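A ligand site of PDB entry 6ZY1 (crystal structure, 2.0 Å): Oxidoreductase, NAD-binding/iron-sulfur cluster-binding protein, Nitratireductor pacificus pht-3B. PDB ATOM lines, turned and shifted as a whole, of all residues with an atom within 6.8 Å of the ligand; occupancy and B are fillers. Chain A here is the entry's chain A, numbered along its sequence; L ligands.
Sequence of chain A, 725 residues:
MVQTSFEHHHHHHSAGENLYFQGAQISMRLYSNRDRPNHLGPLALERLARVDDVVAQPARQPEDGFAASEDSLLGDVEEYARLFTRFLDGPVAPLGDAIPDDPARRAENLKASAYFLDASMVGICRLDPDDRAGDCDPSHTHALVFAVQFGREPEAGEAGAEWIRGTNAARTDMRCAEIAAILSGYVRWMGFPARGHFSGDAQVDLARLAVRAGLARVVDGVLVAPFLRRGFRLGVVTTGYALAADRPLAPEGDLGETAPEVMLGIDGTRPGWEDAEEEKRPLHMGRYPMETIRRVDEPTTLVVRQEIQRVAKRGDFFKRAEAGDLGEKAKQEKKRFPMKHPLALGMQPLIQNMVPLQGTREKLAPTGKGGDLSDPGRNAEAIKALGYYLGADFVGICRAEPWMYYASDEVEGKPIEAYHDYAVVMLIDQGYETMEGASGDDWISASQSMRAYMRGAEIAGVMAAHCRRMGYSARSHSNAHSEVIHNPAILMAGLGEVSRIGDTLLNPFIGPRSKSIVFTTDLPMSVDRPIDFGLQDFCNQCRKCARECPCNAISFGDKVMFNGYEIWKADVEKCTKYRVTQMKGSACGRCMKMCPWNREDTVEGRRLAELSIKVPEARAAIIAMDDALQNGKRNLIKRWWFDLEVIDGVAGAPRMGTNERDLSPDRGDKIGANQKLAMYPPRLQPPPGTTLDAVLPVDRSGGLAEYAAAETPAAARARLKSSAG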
ATOM      1  N   SER A 499      12.420  16.914 -24.450  1.00  0.00           N
ATOM      2  CA  SER A 499      11.444  16.146 -25.203  1.00  0.00           C
ATOM      3  C   SER A 499      11.522  14.679 -24.794  1.00  0.00           C
ATOM      4  O   SER A 499      12.518  14.237 -24.209  1.00  0.00           O
ATOM      5  CB  SER A 499      11.674  16.263 -26.705  1.00  0.00           C
ATOM      6  OG  SER A 499      12.806  15.500 -27.089  1.00  0.00           O
ATOM      7  N   ARG A 500      10.474  13.923 -25.111  1.00  0.00           N
ATOM      8  CA  ARG A 500      10.445  12.516 -24.710  1.00  0.00           C
ATOM      9  C   ARG A 500      11.586  11.732 -25.324  1.00  0.00           C
ATOM     10  O   ARG A 500      12.028  10.728 -24.745  1.00  0.00           O
ATOM     11  CB  ARG A 500       9.115  11.882 -25.085  1.00  0.00           C
ATOM     12  CG  ARG A 500       9.070  10.384 -24.813  1.00  0.00           C
ATOM     13  CD  ARG A 500       7.732   9.778 -25.190  1.00  0.00           C
ATOM     14  NE  ARG A 500       6.633  10.456 -24.517  1.00  0.00           N
ATOM     15  CZ  ARG A 500       6.309  10.263 -23.238  1.00  0.00           C
ATOM     16  NH1 ARG A 500       7.017   9.416 -22.503  1.00  0.00           N
ATOM     17  NH2 ARG A 500       5.295  10.922 -22.706  1.00  0.00           N
ATOM     18  N   ILE A 501      12.086  12.151 -26.492  1.00  0.00           N
ATOM     19  CA  ILE A 501      13.148  11.375 -27.139  1.00  0.00           C
ATOM     20  C   ILE A 501      14.298  11.126 -26.186  1.00  0.00           C
ATOM     21  O   ILE A 501      15.040  10.135 -26.330  1.00  0.00           O
ATOM     22  CB  ILE A 501      13.632  12.067 -28.425  1.00  0.00           C
ATOM     23  CG1 ILE A 501      12.514  12.106 -29.452  1.00  0.00           C
ATOM     24  CG2 ILE A 501      14.844  11.339 -28.987  1.00  0.00           C
ATOM     25  CD1 ILE A 501      12.886  12.849 -30.714  1.00  0.00           C
ATOM     26  N   GLY A 502      14.496  12.010 -25.220  1.00  0.00           N
ATOM     27  CA  GLY A 502      15.415  11.724 -24.132  1.00  0.00           C
ATOM     28  C   GLY A 502      16.662  12.573 -24.149  1.00  0.00           C
ATOM     29  O   GLY A 502      16.721  13.631 -23.516  1.00  0.00           O
ATOM     30  N   THR A 504      17.683  14.165 -26.658  1.00  0.00           N
ATOM     31  CA  THR A 504      17.502  15.111 -27.750  1.00  0.00           C
ATOM     32  C   THR A 504      16.556  16.199 -27.271  1.00  0.00           C
ATOM     33  O   THR A 504      15.513  15.895 -26.691  1.00  0.00           O
ATOM     34  CB  THR A 504      16.921  14.456 -29.003  1.00  0.00           C
ATOM     35  OG1 THR A 504      17.808  13.429 -29.457  1.00  0.00           O
ATOM     36  CG2 THR A 504      16.754  15.467 -30.101  1.00  0.00           C
ATOM     37  N   LEU A 506      14.084  19.464 -28.333  1.00  0.00           N
ATOM     38  CA  LEU A 506      13.158  19.662 -29.437  1.00  0.00           C
ATOM     39  C   LEU A 506      12.895  21.143 -29.626  1.00  0.00           C
ATOM     40  O   LEU A 506      12.515  21.840 -28.678  1.00  0.00           O
ATOM     41  CB  LEU A 506      11.861  18.891 -29.182  1.00  0.00           C
ATOM     42  CG  LEU A 506      10.866  18.687 -30.323  1.00  0.00           C
ATOM     43  CD1 LEU A 506      10.002  17.504 -30.001  1.00  0.00           C
ATOM     44  CD2 LEU A 506      10.014  19.923 -30.517  1.00  0.00           C
ATOM     45  N   PRO A 512      12.943  17.941 -33.562  1.00  0.00           N
ATOM     46  CA  PRO A 512      14.216  17.332 -33.146  1.00  0.00           C
ATOM     47  C   PRO A 512      15.220  17.122 -34.271  1.00  0.00           C
ATOM     48  O   PRO A 512      16.227  16.441 -34.054  1.00  0.00           O
ATOM     49  CB  PRO A 512      13.764  15.975 -32.605  1.00  0.00           C
ATOM     50  CG  PRO A 512      12.603  15.623 -33.488  1.00  0.00           C
ATOM     51  CD  PRO A 512      11.896  16.934 -33.784  1.00  0.00           C
ATOM     52  N   LEU A 535       5.927  22.280 -24.872  1.00  0.00           N
ATOM     53  CA  LEU A 535       6.264  20.922 -25.265  1.00  0.00           C
ATOM     54  C   LEU A 535       6.050  19.920 -24.142  1.00  0.00           C
ATOM     55  O   LEU A 535       5.761  18.748 -24.420  1.00  0.00           O
ATOM     56  CB  LEU A 535       7.710  20.853 -25.734  1.00  0.00           C
ATOM     57  CG  LEU A 535       8.103  19.455 -26.179  1.00  0.00           C
ATOM     58  CD1 LEU A 535       7.332  19.080 -27.445  1.00  0.00           C
ATOM     59  CD2 LEU A 535       9.589  19.372 -26.405  1.00  0.00           C
ATOM     60  N   PHE A 538       2.718  18.704 -24.396  1.00  0.00           N
ATOM     61  CA  PHE A 538       2.556  18.002 -25.670  1.00  0.00           C
ATOM     62  C   PHE A 538       3.201  16.620 -25.614  1.00  0.00           C
ATOM     63  O   PHE A 538       2.552  15.608 -25.940  1.00  0.00           O
ATOM     64  CB  PHE A 538       3.151  18.850 -26.795  1.00  0.00           C
ATOM     65  CG  PHE A 538       2.798  18.351 -28.167  1.00  0.00           C
ATOM     66  CD1 PHE A 538       3.391  17.213 -28.691  1.00  0.00           C
ATOM     67  CD2 PHE A 538       1.878  19.035 -28.947  1.00  0.00           C
ATOM     68  CE1 PHE A 538       3.070  16.752 -29.955  1.00  0.00           C
ATOM     69  CE2 PHE A 538       1.547  18.595 -30.219  1.00  0.00           C
ATOM     70  CZ  PHE A 538       2.138  17.444 -30.725  1.00  0.00           C
ATOM     71  N   CYS A 539       4.475  16.532 -25.227  1.00  0.00           N
ATOM     72  CA  CYS A 539       5.103  15.230 -25.136  1.00  0.00           C
ATOM     73  C   CYS A 539       4.371  14.327 -24.144  1.00  0.00           C
ATOM     74  O   CYS A 539       4.324  13.111 -24.332  1.00  0.00           O
ATOM     75  CB  CYS A 539       6.564  15.348 -24.735  1.00  0.00           C
ATOM     76  SG  CYS A 539       7.654  15.693 -26.120  1.00  0.00           S
ATOM     77  N   ASN A 540       3.774  14.915 -23.108  1.00  0.00           N
ATOM     78  CA  ASN A 540       3.030  14.132 -22.135  1.00  0.00           C
ATOM     79  C   ASN A 540       1.880  13.371 -22.784  1.00  0.00           C
ATOM     80  O   ASN A 540       1.460  12.341 -22.246  1.00  0.00           O
ATOM     81  CB  ASN A 540       2.511  15.045 -21.032  1.00  0.00           C
ATOM     82  CG  ASN A 540       2.431  14.352 -19.686  1.00  0.00           C
ATOM     83  OD1 ASN A 540       1.341  14.149 -19.157  1.00  0.00           O
ATOM     84  ND2 ASN A 540       3.589  13.992 -19.134  1.00  0.00           N
ATOM     85  N   GLN A 541       1.384  13.842 -23.929  1.00  0.00           N
ATOM     86  CA  GLN A 541       0.252  13.222 -24.618  1.00  0.00           C
ATOM     87  C   GLN A 541       0.666  12.462 -25.871  1.00  0.00           C
ATOM     88  O   GLN A 541      -0.207  12.036 -26.639  1.00  0.00           O
ATOM     89  CB  GLN A 541      -0.782  14.281 -25.005  1.00  0.00           C
ATOM     90  CG  GLN A 541      -1.170  15.219 -23.897  1.00  0.00           C
ATOM     91  CD  GLN A 541      -2.261  16.180 -24.337  1.00  0.00           C
ATOM     92  OE1 GLN A 541      -3.193  15.797 -25.038  1.00  0.00           O
ATOM     93  NE2 GLN A 541      -2.136  17.439 -23.929  1.00  0.00           N
ATOM     94  N   CYS A 542       1.958  12.292 -26.114  1.00  0.00           N
ATOM     95  CA  CYS A 542       2.449  11.743 -27.369  1.00  0.00           C
ATOM     96  C   CYS A 542       3.395  10.589 -27.080  1.00  0.00           C
ATOM     97  O   CYS A 542       4.146  10.632 -26.096  1.00  0.00           O
ATOM     98  CB  CYS A 542       3.145  12.822 -28.190  1.00  0.00           C
ATOM     99  SG  CYS A 542       3.605  12.356 -29.851  1.00  0.00           S
ATOM    100  N   ARG A 543       3.350   9.559 -27.925  1.00  0.00           N
ATOM    101  CA  ARG A 543       4.247   8.423 -27.777  1.00  0.00           C
ATOM    102  C   ARG A 543       4.895   7.995 -29.097  1.00  0.00           C
ATOM    103  O   ARG A 543       5.516   6.933 -29.136  1.00  0.00           O
ATOM    104  CB  ARG A 543       3.504   7.214 -27.192  1.00  0.00           C
ATOM    105  CG  ARG A 543       2.856   7.481 -25.845  1.00  0.00           C
ATOM    106  CD  ARG A 543       3.898   7.869 -24.832  1.00  0.00           C
ATOM    107  NE  ARG A 543       3.378   7.849 -23.474  1.00  0.00           N
ATOM    108  CZ  ARG A 543       2.766   8.875 -22.895  1.00  0.00           C
ATOM    109  NH1 ARG A 543       2.586  10.003 -23.565  1.00  0.00           N
ATOM    110  NH2 ARG A 543       2.335   8.772 -21.647  1.00  0.00           N
ATOM    111  N   LYS A 544       4.778   8.794 -30.153  1.00  0.00           N
ATOM    112  CA  LYS A 544       5.155   8.317 -31.479  1.00  0.00           C
ATOM    113  C   LYS A 544       6.615   7.871 -31.536  1.00  0.00           C
ATOM    114  O   LYS A 544       6.917   6.762 -31.992  1.00  0.00           O
ATOM    115  CB  LYS A 544       4.865   9.398 -32.524  1.00  0.00           C
ATOM    116  CG  LYS A 544       4.952   8.894 -33.947  1.00  0.00           C
ATOM    117  CD  LYS A 544       4.163   9.766 -34.891  1.00  0.00           C
ATOM    118  CE  LYS A 544       4.168   9.189 -36.289  1.00  0.00           C
ATOM    119  NZ  LYS A 544       3.135   9.827 -37.155  1.00  0.00           N
ATOM    120  N   CYS A 545       7.534   8.721 -31.076  1.00  0.00           N
ATOM    121  CA  CYS A 545       8.946   8.351 -31.080  1.00  0.00           C
ATOM    122  C   CYS A 545       9.173   7.062 -30.314  1.00  0.00           C
ATOM    123  O   CYS A 545       9.912   6.178 -30.769  1.00  0.00           O
ATOM    124  CB  CYS A 545       9.796   9.480 -30.505  1.00  0.00           C
ATOM    125  SG  CYS A 545       9.302  10.012 -28.852  1.00  0.00           S
ATOM    126  N   ALA A 546       8.566   6.935 -29.140  1.00  0.00           N
ATOM    127  CA  ALA A 546       8.755   5.731 -28.337  1.00  0.00           C
ATOM    128  C   ALA A 546       8.205   4.516 -29.059  1.00  0.00           C
ATOM    129  O   ALA A 546       8.818   3.435 -29.035  1.00  0.00           O
ATOM    130  CB  ALA A 546       8.064   5.900 -26.981  1.00  0.00           C
ATOM    131  N   ILE A 554      13.246   4.480 -26.020  1.00  0.00           N
ATOM    132  CA  ILE A 554      12.612   5.713 -25.574  1.00  0.00           C
ATOM    133  C   ILE A 554      11.520   5.380 -24.579  1.00  0.00           C
ATOM    134  O   ILE A 554      10.777   4.404 -24.747  1.00  0.00           O
ATOM    135  CB  ILE A 554      12.063   6.519 -26.771  1.00  0.00           C
ATOM    136  CG1 ILE A 554      13.176   6.875 -27.753  1.00  0.00           C
ATOM    137  CG2 ILE A 554      11.390   7.788 -26.291  1.00  0.00           C
ATOM    138  CD1 ILE A 554      12.688   7.698 -28.928  1.00  0.00           C
ATOM    139  N   TRP A 568      13.080  13.027 -19.511  1.00  0.00           N
ATOM    140  CA  TRP A 568      12.718  11.696 -19.993  1.00  0.00           C
ATOM    141  C   TRP A 568      14.009  10.971 -20.332  1.00  0.00           C
ATOM    142  O   TRP A 568      14.699  11.342 -21.299  1.00  0.00           O
ATOM    143  CB  TRP A 568      11.824  11.773 -21.237  1.00  0.00           C
ATOM    144  CG  TRP A 568      10.360  12.012 -20.972  1.00  0.00           C
ATOM    145  CD1 TRP A 568       9.456  11.127 -20.452  1.00  0.00           C
ATOM    146  CD2 TRP A 568       9.630  13.214 -21.267  1.00  0.00           C
ATOM    147  NE1 TRP A 568       8.215  11.702 -20.392  1.00  0.00           N
ATOM    148  CE2 TRP A 568       8.289  12.981 -20.878  1.00  0.00           C
ATOM    149  CE3 TRP A 568       9.978  14.443 -21.803  1.00  0.00           C
ATOM    150  CZ2 TRP A 568       7.304  13.956 -21.017  1.00  0.00           C
ATOM    151  CZ3 TRP A 568       8.997  15.409 -21.932  1.00  0.00           C
ATOM    152  CH2 TRP A 568       7.683  15.159 -21.547  1.00  0.00           C
ATOM    153  N   CYS A 591      13.853   8.262 -34.537  1.00  0.00           N
ATOM    154  CA  CYS A 591      12.991   9.016 -33.642  1.00  0.00           C
ATOM    155  C   CYS A 591      12.825  10.460 -34.107  1.00  0.00           C
ATOM    156  O   CYS A 591      11.726  11.022 -34.030  1.00  0.00           O
ATOM    157  CB  CYS A 591      13.543   8.963 -32.221  1.00  0.00           C
ATOM    158  SG  CYS A 591      15.336   9.096 -32.113  1.00  0.00           S
ATOM    159  N   MET A 594      10.169  10.375 -36.949  1.00  0.00           N
ATOM    160  CA  MET A 594       8.779  10.053 -36.629  1.00  0.00           C
ATOM    161  C   MET A 594       8.080  11.143 -35.831  1.00  0.00           C
ATOM    162  O   MET A 594       6.843  11.106 -35.724  1.00  0.00           O
ATOM    163  CB  MET A 594       8.708   8.739 -35.858  1.00  0.00           C
ATOM    164  CG  MET A 594       9.140   7.508 -36.643  1.00  0.00           C
ATOM    165  SD  MET A 594       8.223   7.287 -38.180  1.00  0.00           S
ATOM    166  CE  MET A 594       9.496   7.637 -39.365  1.00  0.00           C
ATOM    167  N   CYS A 595       8.806  12.109 -35.285  1.00  0.00           N
ATOM    168  CA  CYS A 595       8.192  13.064 -34.391  1.00  0.00           C
ATOM    169  C   CYS A 595       7.232  13.970 -35.162  1.00  0.00           C
ATOM    170  O   CYS A 595       7.555  14.435 -36.258  1.00  0.00           O
ATOM    171  CB  CYS A 595       9.250  13.910 -33.686  1.00  0.00           C
ATOM    172  SG  CYS A 595       8.578  15.130 -32.559  1.00  0.00           S
ATOM    173  N   PRO A 596       6.044  14.247 -34.605  1.00  0.00           N
ATOM    174  CA  PRO A 596       5.108  15.132 -35.307  1.00  0.00           C
ATOM    175  C   PRO A 596       5.678  16.519 -35.556  1.00  0.00           C
ATOM    176  O   PRO A 596       5.268  17.178 -36.523  1.00  0.00           O
ATOM    177  CB  PRO A 596       3.894  15.182 -34.369  1.00  0.00           C
ATOM    178  CG  PRO A 596       4.005  13.956 -33.509  1.00  0.00           C
ATOM    179  CD  PRO A 596       5.488  13.707 -33.359  1.00  0.00           C
ATOM    180  N   TRP A 597       6.612  16.970 -34.722  1.00  0.00           N
ATOM    181  CA  TRP A 597       7.252  18.264 -34.940  1.00  0.00           C
ATOM    182  C   TRP A 597       8.220  18.249 -36.108  1.00  0.00           C
ATOM    183  O   TRP A 597       8.671  19.318 -36.537  1.00  0.00           O
ATOM    184  CB  TRP A 597       7.968  18.697 -33.662  1.00  0.00           C
ATOM    185  CG  TRP A 597       7.025  18.979 -32.536  1.00  0.00           C
ATOM    186  CD1 TRP A 597       6.458  18.067 -31.694  1.00  0.00           C
ATOM    187  CD2 TRP A 597       6.517  20.264 -32.137  1.00  0.00           C
ATOM    188  NE1 TRP A 597       5.640  18.705 -30.797  1.00  0.00           N
ATOM    189  CE2 TRP A 597       5.655  20.051 -31.044  1.00  0.00           C
ATOM    190  CE3 TRP A 597       6.717  21.571 -32.604  1.00  0.00           C
ATOM    191  CZ2 TRP A 597       4.997  21.095 -30.405  1.00  0.00           C
ATOM    192  CZ3 TRP A 597       6.054  22.611 -31.957  1.00  0.00           C
ATOM    193  CH2 TRP A 597       5.211  22.361 -30.874  1.00  0.00           C
ATOM    194  N   ASN A 598       8.550  17.082 -36.633  1.00  0.00           N
ATOM    195  CA  ASN A 598       9.321  16.965 -37.868  1.00  0.00           C
ATOM    196  C   ASN A 598       8.373  17.192 -39.035  1.00  0.00           C
ATOM    197  O   ASN A 598       7.692  16.264 -39.478  1.00  0.00           O
ATOM    198  CB  ASN A 598       9.991  15.601 -37.930  1.00  0.00           C
ATOM    199  CG  ASN A 598      10.827  15.422 -39.172  1.00  0.00           C
ATOM    200  OD1 ASN A 598      11.570  16.313 -39.556  1.00  0.00           O
ATOM    201  ND2 ASN A 598      10.708  14.265 -39.821  1.00  0.00           N
ATOM    202  N   ILE A 623      -1.714  15.174 -32.369  1.00  0.00           N
ATOM    203  CA  ILE A 623      -0.952  13.955 -32.130  1.00  0.00           C
ATOM    204  C   ILE A 623      -1.647  12.760 -32.776  1.00  0.00           C
ATOM    205  O   ILE A 623      -0.973  11.862 -33.307  1.00  0.00           O
ATOM    206  CB  ILE A 623      -0.757  13.759 -30.611  1.00  0.00           C
ATOM    207  CG1 ILE A 623       0.098  14.892 -30.044  1.00  0.00           C
ATOM    208  CG2 ILE A 623      -0.097  12.455 -30.341  1.00  0.00           C
ATOM    209  CD1 ILE A 623       0.050  15.007 -28.543  1.00  0.00           C
HETATM  210 FE1  LIG L   1       8.232  11.997 -28.942  1.00  0.00          FE
HETATM  211 FE2  LIG L   1       5.780  12.968 -29.566  1.00  0.00          FE
HETATM  212 FE3  LIG L   1       8.011  14.152 -30.607  1.00  0.00          FE
HETATM  213 FE4  LIG L   1       7.444  14.422 -27.964  1.00  0.00          FE
HETATM  214  S1  LIG L   1       6.225  15.206 -29.724  1.00  0.00           S
HETATM  215  S2  LIG L   1       9.455  13.918 -28.860  1.00  0.00           S
HETATM  216  S3  LIG L   1       6.529  12.382 -27.505  1.00  0.00           S
HETATM  217  S4  LIG L   1       7.256  12.025 -30.994  1.00  0.00           S
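The backbone carbonyl oxygen (O) of Cys 542 is in hydrogen-bond range of the guanidinium group (NE) of Arg 500 (3.0 Å). The backbone NH (N) of Trp 597 sits close to the side-chain sulfur (SG) of Cys 595 (3.5 Å). N of Ile 501 lies close to OG of Ser 499. NH2 of Arg 500 lies within hydrogen-bond range of O of Cys 539. The side-chain sulfur (SG) of Cys 542 sits close to the backbone NH (N) of Lys 544, 3.8 Å away. OG of Ser 499 is in hydrogen-bond range of O of Thr 504, 2.8 Å away.
The side-chain sulfur (SG) of Cys 539 binds an iron atom (FE4) of the ligand (2.2 Å). NE1 of Trp 597 sits close to S1 of the ligand (3.7 Å). SG of Cys 545 binds FE1 of the ligand, at 2.3 Å. N of Cys 545 lies close to S4 of the ligand, at 3.3 Å. A sulfur (S3) of the ligand sits close to the guanidinium group (NE) of Arg 500 (3.6 Å). The side-chain sulfur (SG) of Cys 595 binds an iron atom (FE3) of the ligand, 2.3 Å away. The side-chain sulfur (SG) of Cys 542 is bound to an iron atom (FE2) of the ligand, at 2.3 Å.
Ser 499 touches the ligand (CB to S2, 3.9 Å). Ile 501 touches the ligand (CG1 to S2, 3.6 Å). CD1 of Leu 506 touches S2 of the ligand, 3.8 Å away. Phe 538 touches the ligand (CE1 to S1, 3.5 Å). CB of Lys 544 touches S4 of the ligand, at 3.9 Å. Pro 596 touches the ligand. Hydrophobic or aromatic side chains that line the ligand: Ile 501, Leu 506, Phe 538, Pro 596 and Trp 597.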
